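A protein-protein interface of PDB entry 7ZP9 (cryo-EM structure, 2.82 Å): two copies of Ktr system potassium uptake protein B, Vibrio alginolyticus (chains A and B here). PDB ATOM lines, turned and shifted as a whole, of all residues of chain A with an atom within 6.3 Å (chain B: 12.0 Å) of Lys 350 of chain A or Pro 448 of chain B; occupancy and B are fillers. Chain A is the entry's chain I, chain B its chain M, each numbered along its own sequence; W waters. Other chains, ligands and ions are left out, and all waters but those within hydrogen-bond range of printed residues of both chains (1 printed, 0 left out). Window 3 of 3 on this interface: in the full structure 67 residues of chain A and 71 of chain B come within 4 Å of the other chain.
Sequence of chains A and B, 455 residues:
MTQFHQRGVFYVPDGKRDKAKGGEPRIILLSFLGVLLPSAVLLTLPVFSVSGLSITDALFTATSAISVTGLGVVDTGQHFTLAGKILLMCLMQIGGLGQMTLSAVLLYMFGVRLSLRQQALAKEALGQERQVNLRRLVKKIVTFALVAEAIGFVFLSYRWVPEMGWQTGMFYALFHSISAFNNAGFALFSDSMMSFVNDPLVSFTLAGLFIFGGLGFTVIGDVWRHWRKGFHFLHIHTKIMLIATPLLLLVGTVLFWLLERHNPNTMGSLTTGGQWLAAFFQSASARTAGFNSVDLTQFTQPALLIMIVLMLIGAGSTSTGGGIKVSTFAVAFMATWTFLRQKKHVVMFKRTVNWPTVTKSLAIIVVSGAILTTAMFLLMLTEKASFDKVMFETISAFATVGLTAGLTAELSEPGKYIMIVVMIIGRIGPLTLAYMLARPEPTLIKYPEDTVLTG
N of Asp 450 of chain B lies within hydrogen-bond range of O of Thr 352 of chain A, at 3.1 Å.
The backbone carbonyl oxygen (O) of Tyr 447 of chain B sits at hydrogen-bond distance from the side-chain hydroxyl (OG1) of Thr 352 of chain A.
NH1 of Arg 351 of chain A is in salt-bridge range of OD2 of Asp 450 of chain B, 3.5 Å away.
The backbone NH (N) of Thr 352 of chain A is in hydrogen-bond range of the backbone carbonyl oxygen (O) of Pro 448 of chain B.
The side-chain amino group (NZ) of Lys 350 of chain A is in hydrogen-bond range of the side-chain hydroxyl (OH) of Tyr 447 of chain B (3.4 Å).
Val 347 of chain A touches Tyr 447 of chain B (CG1 to CD2, 3.7 Å).
CD of Pro 448 of chain B touches O of Lys 350 of chain A, at 3.9 Å.
Tyr 447 of chain B touches Arg 351 of chain A (CB to CA, 3.9 Å).
Arg 351 of chain A touches Pro 448 of chain B (CA to O, 3.4 Å).
Thr 352 of chain A touches Lys 446 of chain B.
Glu 449 of chain B touches Thr 352 of chain A (CA to O, 3.3 Å).
Of chain B, only Tyr 447 (3.7 Å) comes within 4 Å of Val 347 of chain A.
No residue of chain B comes within 4 Å of Phe 349 of chain A.
Lys 350 of chain A touches just these residues of chain B: Tyr 447 (3.2 Å) and Pro 448 (3.9 Å).
Printed residues of chain B within 4 Å of Arg 351 of chain A: Tyr 447, Pro 448 and Asp 450.
Val 353 of chain A touches none of the printed residues of chain B.
Leu 444 of chain B touches none of the printed residues of chain A.
Of the printed residues of chain A, Lys 446 of chain B touches Thr 352.
Of the printed residues of chain A, Tyr 447 of chain B touches Val 347 (3.7 Å), Lys 350 (3.2 Å), Arg 351 (3.9 Å) and Thr 352 (2.7 Å).
Of the printed residues of chain A, Pro 448 of chain B touches Lys 350, Arg 351 and Thr 352.
Of the printed residues of chain A, Glu 449 of chain B touches Thr 352 (3.3 Å).
Of the printed residues of chain A, Asp 450 of chain B touches Arg 351 and Thr 352.
The nearest printed residue of chain B that does not touch Arg 351 of chain A is Glu 449 of chain B (5.2 Å).
Printed residues of chain B that touch a printed residue of chain A: Lys 446, Tyr 447, Pro 448, Glu 449 and Asp 450.
Hydrophobic or aromatic side chains of chain B within 4 Å of the printed part of chain A: Tyr 447 and Pro 448.
Along chain A the printed residues that touch a printed residue of chain B span positions 347 to 352.
Among the printed residues, 11 pairs touch across the chains.
Among the printed residues, Asp or Glu carboxylates within 4 Å of a Lys or Arg side-chain nitrogen of the other chain: Arg 351 of chain A with Asp 450 of chain B (3.5 Å).
No position is printed for both chains.
Of the 11 pairs that touch across the chains among the printed residues, none has its exchanged pair printed and touching as well.
Water W1 lies within hydrogen-bond range of OG1 of Thr 352 of chain A (3.1 Å) and N of Tyr 447 of chain B (3.2 Å).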
ATOM      1  N   HIS A 232     -33.566 -11.019 -29.799  1.00  0.00           N
ATOM      2  CA  HIS A 232     -33.336 -11.155 -28.366  1.00  0.00           C
ATOM      3  C   HIS A 232     -34.317 -12.121 -27.717  1.00  0.00           C
ATOM      4  O   HIS A 232     -33.981 -12.765 -26.717  1.00  0.00           O
ATOM      5  CB  HIS A 232     -33.420  -9.784 -27.696  1.00  0.00           C
ATOM      6  CG  HIS A 232     -33.111  -9.804 -26.234  1.00  0.00           C
ATOM      7  ND1 HIS A 232     -31.852  -9.551 -25.736  1.00  0.00           N
ATOM      8  CD2 HIS A 232     -33.900 -10.037 -25.158  1.00  0.00           C
ATOM      9  CE1 HIS A 232     -31.876  -9.633 -24.418  1.00  0.00           C
ATOM     10  NE2 HIS A 232     -33.108  -9.927 -24.043  1.00  0.00           N
ATOM     11  N   VAL A 347     -22.996 -20.409 -19.365  1.00  0.00           N
ATOM     12  CA  VAL A 347     -23.937 -19.356 -19.726  1.00  0.00           C
ATOM     13  C   VAL A 347     -23.860 -19.137 -21.228  1.00  0.00           C
ATOM     14  O   VAL A 347     -22.771 -18.929 -21.776  1.00  0.00           O
ATOM     15  CB  VAL A 347     -23.643 -18.049 -18.970  1.00  0.00           C
ATOM     16  CG1 VAL A 347     -24.496 -16.917 -19.515  1.00  0.00           C
ATOM     17  CG2 VAL A 347     -23.880 -18.235 -17.485  1.00  0.00           C
ATOM     18  N   MET A 348     -25.013 -19.187 -21.890  1.00  0.00           N
ATOM     19  CA  MET A 348     -25.105 -18.955 -23.325  1.00  0.00           C
ATOM     20  C   MET A 348     -26.277 -18.022 -23.580  1.00  0.00           C
ATOM     21  O   MET A 348     -27.420 -18.364 -23.259  1.00  0.00           O
ATOM     22  CB  MET A 348     -25.284 -20.272 -24.082  1.00  0.00           C
ATOM     23  CG  MET A 348     -24.074 -21.180 -23.995  1.00  0.00           C
ATOM     24  SD  MET A 348     -24.273 -22.775 -24.804  1.00  0.00           S
ATOM     25  CE  MET A 348     -24.267 -22.272 -26.519  1.00  0.00           C
ATOM     26  N   PHE A 349     -25.995 -16.849 -24.149  1.00  0.00           N
ATOM     27  CA  PHE A 349     -27.013 -15.832 -24.418  1.00  0.00           C
ATOM     28  C   PHE A 349     -27.785 -15.475 -23.149  1.00  0.00           C
ATOM     29  O   PHE A 349     -29.016 -15.419 -23.136  1.00  0.00           O
ATOM     30  CB  PHE A 349     -27.963 -16.280 -25.531  1.00  0.00           C
ATOM     31  CG  PHE A 349     -27.287 -16.502 -26.847  1.00  0.00           C
ATOM     32  CD1 PHE A 349     -27.017 -15.438 -27.689  1.00  0.00           C
ATOM     33  CD2 PHE A 349     -26.921 -17.773 -27.246  1.00  0.00           C
ATOM     34  CE1 PHE A 349     -26.394 -15.639 -28.899  1.00  0.00           C
ATOM     35  CE2 PHE A 349     -26.296 -17.978 -28.456  1.00  0.00           C
ATOM     36  CZ  PHE A 349     -26.033 -16.909 -29.283  1.00  0.00           C
ATOM     37  N   LYS A 350     -27.040 -15.241 -22.068  1.00  0.00           N
ATOM     38  CA  LYS A 350     -27.600 -14.857 -20.771  1.00  0.00           C
ATOM     39  C   LYS A 350     -28.536 -15.923 -20.211  1.00  0.00           C
ATOM     40  O   LYS A 350     -29.489 -15.608 -19.497  1.00  0.00           O
ATOM     41  CB  LYS A 350     -28.321 -13.507 -20.849  1.00  0.00           C
ATOM     42  CG  LYS A 350     -27.462 -12.361 -21.347  1.00  0.00           C
ATOM     43  CD  LYS A 350     -26.384 -11.999 -20.345  1.00  0.00           C
ATOM     44  CE  LYS A 350     -25.485 -10.902 -20.887  1.00  0.00           C
ATOM     45  NZ  LYS A 350     -24.396 -10.559 -19.934  1.00  0.00           N
ATOM     46  N   ARG A 351     -28.284 -17.188 -20.537  1.00  0.00           N
ATOM     47  CA  ARG A 351     -29.063 -18.303 -20.012  1.00  0.00           C
ATOM     48  C   ARG A 351     -28.111 -19.375 -19.513  1.00  0.00           C
ATOM     49  O   ARG A 351     -27.134 -19.699 -20.193  1.00  0.00           O
ATOM     50  CB  ARG A 351     -29.994 -18.895 -21.075  1.00  0.00           C
ATOM     51  CG  ARG A 351     -31.064 -17.953 -21.585  1.00  0.00           C
ATOM     52  CD  ARG A 351     -32.136 -17.700 -20.543  1.00  0.00           C
ATOM     53  NE  ARG A 351     -32.824 -16.441 -20.796  1.00  0.00           N
ATOM     54  CZ  ARG A 351     -33.987 -16.337 -21.422  1.00  0.00           C
ATOM     55  NH1 ARG A 351     -34.641 -17.405 -21.846  1.00  0.00           N
ATOM     56  NH2 ARG A 351     -34.506 -15.131 -21.629  1.00  0.00           N
ATOM     57  N   THR A 352     -28.397 -19.923 -18.338  1.00  0.00           N
ATOM     58  CA  THR A 352     -27.579 -21.004 -17.807  1.00  0.00           C
ATOM     59  C   THR A 352     -27.915 -22.310 -18.514  1.00  0.00           C
ATOM     60  O   THR A 352     -29.087 -22.674 -18.645  1.00  0.00           O
ATOM     61  CB  THR A 352     -27.795 -21.148 -16.303  1.00  0.00           C
ATOM     62  OG1 THR A 352     -27.501 -19.907 -15.655  1.00  0.00           O
ATOM     63  CG2 THR A 352     -26.900 -22.232 -15.738  1.00  0.00           C
ATOM     64  N   VAL A 353     -26.887 -23.010 -18.976  1.00  0.00           N
ATOM     65  CA  VAL A 353     -27.048 -24.346 -19.532  1.00  0.00           C
ATOM     66  C   VAL A 353     -26.942 -25.346 -18.392  1.00  0.00           C
ATOM     67  O   VAL A 353     -25.904 -25.434 -17.725  1.00  0.00           O
ATOM     68  CB  VAL A 353     -25.995 -24.625 -20.617  1.00  0.00           C
ATOM     69  CG1 VAL A 353     -26.161 -26.027 -21.172  1.00  0.00           C
ATOM     70  CG2 VAL A 353     -26.096 -23.595 -21.726  1.00  0.00           C
ATOM     71  N   THR B 443     -20.372 -17.253  -7.645  1.00  0.00           N
ATOM     72  CA  THR B 443     -21.011 -16.121  -8.296  1.00  0.00           C
ATOM     73  C   THR B 443     -22.236 -15.678  -7.507  1.00  0.00           C
ATOM     74  O   THR B 443     -22.826 -16.445  -6.740  1.00  0.00           O
ATOM     75  CB  THR B 443     -21.409 -16.470  -9.734  1.00  0.00           C
ATOM     76  OG1 THR B 443     -21.781 -15.278 -10.436  1.00  0.00           O
ATOM     77  CG2 THR B 443     -22.577 -17.446  -9.746  1.00  0.00           C
ATOM     78  N   LEU B 444     -22.603 -14.413  -7.695  1.00  0.00           N
ATOM     79  CA  LEU B 444     -23.796 -13.853  -7.079  1.00  0.00           C
ATOM     80  C   LEU B 444     -24.934 -13.663  -8.069  1.00  0.00           C
ATOM     81  O   LEU B 444     -26.070 -13.431  -7.644  1.00  0.00           O
ATOM     82  CB  LEU B 444     -23.467 -12.512  -6.413  1.00  0.00           C
ATOM     83  CG  LEU B 444     -22.369 -12.567  -5.351  1.00  0.00           C
ATOM     84  CD1 LEU B 444     -21.919 -11.170  -4.964  1.00  0.00           C
ATOM     85  CD2 LEU B 444     -22.844 -13.340  -4.135  1.00  0.00           C
ATOM     86  N   ILE B 445     -24.661 -13.765  -9.364  1.00  0.00           N
ATOM     87  CA  ILE B 445     -25.660 -13.591 -10.411  1.00  0.00           C
ATOM     88  C   ILE B 445     -25.793 -14.908 -11.156  1.00  0.00           C
ATOM     89  O   ILE B 445     -24.810 -15.427 -11.699  1.00  0.00           O
ATOM     90  CB  ILE B 445     -25.280 -12.454 -11.372  1.00  0.00           C
ATOM     91  CG1 ILE B 445     -25.336 -11.102 -10.659  1.00  0.00           C
ATOM     92  CG2 ILE B 445     -26.176 -12.465 -12.595  1.00  0.00           C
ATOM     93  CD1 ILE B 445     -26.556 -10.914  -9.795  1.00  0.00           C
ATOM     94  N   LYS B 446     -27.005 -15.450 -11.185  1.00  0.00           N
ATOM     95  CA  LYS B 446     -27.315 -16.634 -11.969  1.00  0.00           C
ATOM     96  C   LYS B 446     -28.385 -16.299 -12.996  1.00  0.00           C
ATOM     97  O   LYS B 446     -29.367 -15.620 -12.686  1.00  0.00           O
ATOM     98  CB  LYS B 446     -27.792 -17.786 -11.083  1.00  0.00           C
ATOM     99  CG  LYS B 446     -28.021 -19.074 -11.848  1.00  0.00           C
ATOM    100  CD  LYS B 446     -28.292 -20.243 -10.926  1.00  0.00           C
ATOM    101  CE  LYS B 446     -28.612 -21.491 -11.726  1.00  0.00           C
ATOM    102  NZ  LYS B 446     -28.204 -22.730 -11.012  1.00  0.00           N
ATOM    103  N   TYR B 447     -28.185 -16.762 -14.209  1.00  0.00           N
ATOM    104  CA  TYR B 447     -29.161 -16.569 -15.264  1.00  0.00           C
ATOM    105  C   TYR B 447     -30.143 -17.731 -15.291  1.00  0.00           C
ATOM    106  O   TYR B 447     -29.832 -18.830 -14.822  1.00  0.00           O
ATOM    107  CB  TYR B 447     -28.451 -16.430 -16.605  1.00  0.00           C
ATOM    108  CG  TYR B 447     -27.556 -15.218 -16.672  1.00  0.00           C
ATOM    109  CD1 TYR B 447     -28.091 -13.945 -16.800  1.00  0.00           C
ATOM    110  CD2 TYR B 447     -26.177 -15.344 -16.604  1.00  0.00           C
ATOM    111  CE1 TYR B 447     -27.279 -12.834 -16.857  1.00  0.00           C
ATOM    112  CE2 TYR B 447     -25.358 -14.238 -16.663  1.00  0.00           C
ATOM    113  CZ  TYR B 447     -25.914 -12.986 -16.790  1.00  0.00           C
ATOM    114  OH  TYR B 447     -25.100 -11.879 -16.849  1.00  0.00           O
ATOM    115  N   PRO B 448     -31.353 -17.517 -15.810  1.00  0.00           N
ATOM    116  CA  PRO B 448     -32.342 -18.599 -15.828  1.00  0.00           C
ATOM    117  C   PRO B 448     -31.859 -19.781 -16.654  1.00  0.00           C
ATOM    118  O   PRO B 448     -31.187 -19.619 -17.673  1.00  0.00           O
ATOM    119  CB  PRO B 448     -33.579 -17.946 -16.455  1.00  0.00           C
ATOM    120  CG  PRO B 448     -33.337 -16.491 -16.398  1.00  0.00           C
ATOM    121  CD  PRO B 448     -31.868 -16.292 -16.440  1.00  0.00           C
ATOM    122  N   GLU B 449     -32.209 -20.979 -16.200  1.00  0.00           N
ATOM    123  CA  GLU B 449     -31.865 -22.185 -16.936  1.00  0.00           C
ATOM    124  C   GLU B 449     -32.759 -22.320 -18.157  1.00  0.00           C
ATOM    125  O   GLU B 449     -33.982 -22.180 -18.064  1.00  0.00           O
ATOM    126  CB  GLU B 449     -32.006 -23.413 -16.039  1.00  0.00           C
ATOM    127  CG  GLU B 449     -30.726 -23.829 -15.347  1.00  0.00           C
ATOM    128  CD  GLU B 449     -30.898 -25.090 -14.527  1.00  0.00           C
ATOM    129  OE1 GLU B 449     -31.995 -25.683 -14.574  1.00  0.00           O
ATOM    130  OE2 GLU B 449     -29.938 -25.490 -13.834  1.00  0.00           O
ATOM    131  N   ASP B 450     -32.150 -22.584 -19.307  1.00  0.00           N
ATOM    132  CA  ASP B 450     -32.889 -22.816 -20.535  1.00  0.00           C
ATOM    133  C   ASP B 450     -32.336 -24.056 -21.220  1.00  0.00           C
ATOM    134  O   ASP B 450     -31.155 -24.388 -21.094  1.00  0.00           O
ATOM    135  CB  ASP B 450     -32.821 -21.608 -21.476  1.00  0.00           C
ATOM    136  CG  ASP B 450     -33.974 -21.574 -22.458  1.00  0.00           C
ATOM    137  OD1 ASP B 450     -34.781 -22.527 -22.459  1.00  0.00           O
ATOM    138  OD2 ASP B 450     -34.082 -20.593 -23.224  1.00  0.00           O
ATOM    139  N   THR B 451     -33.195 -24.693 -22.000  1.00  0.00           N
ATOM    140  CA  THR B 451     -32.796 -25.969 -22.630  1.00  0.00           C
ATOM    141  C   THR B 451     -32.193 -25.767 -24.011  1.00  0.00           C
ATOM    142  O   THR B 451     -32.712 -24.940 -24.766  1.00  0.00           O
ATOM    143  CB  THR B 451     -34.000 -26.911 -22.743  1.00  0.00           C
ATOM    144  OG1 THR B 451     -33.604 -28.050 -23.503  1.00  0.00           O
ATOM    145  CG2 THR B 451     -35.202 -26.249 -23.382  1.00  0.00           C
ATOM    146  N   VAL B 452     -31.156 -26.542 -24.313  1.00  0.00           N
ATOM    147  CA  VAL B 452     -30.583 -26.522 -25.683  1.00  0.00           C
ATOM    148  C   VAL B 452     -30.752 -27.939 -26.219  1.00  0.00           C
ATOM    149  O   VAL B 452     -30.504 -28.876 -25.465  1.00  0.00           O
ATOM    150  CB  VAL B 452     -29.126 -26.015 -25.731  1.00  0.00           C
ATOM    151  CG1 VAL B 452     -28.579 -25.971 -27.144  1.00  0.00           C
ATOM    152  CG2 VAL B 452     -28.967 -24.676 -25.036  1.00  0.00           C
HETATM  153  O   HOH W   1     -25.272 -18.141 -14.479  1.00  0.00           O
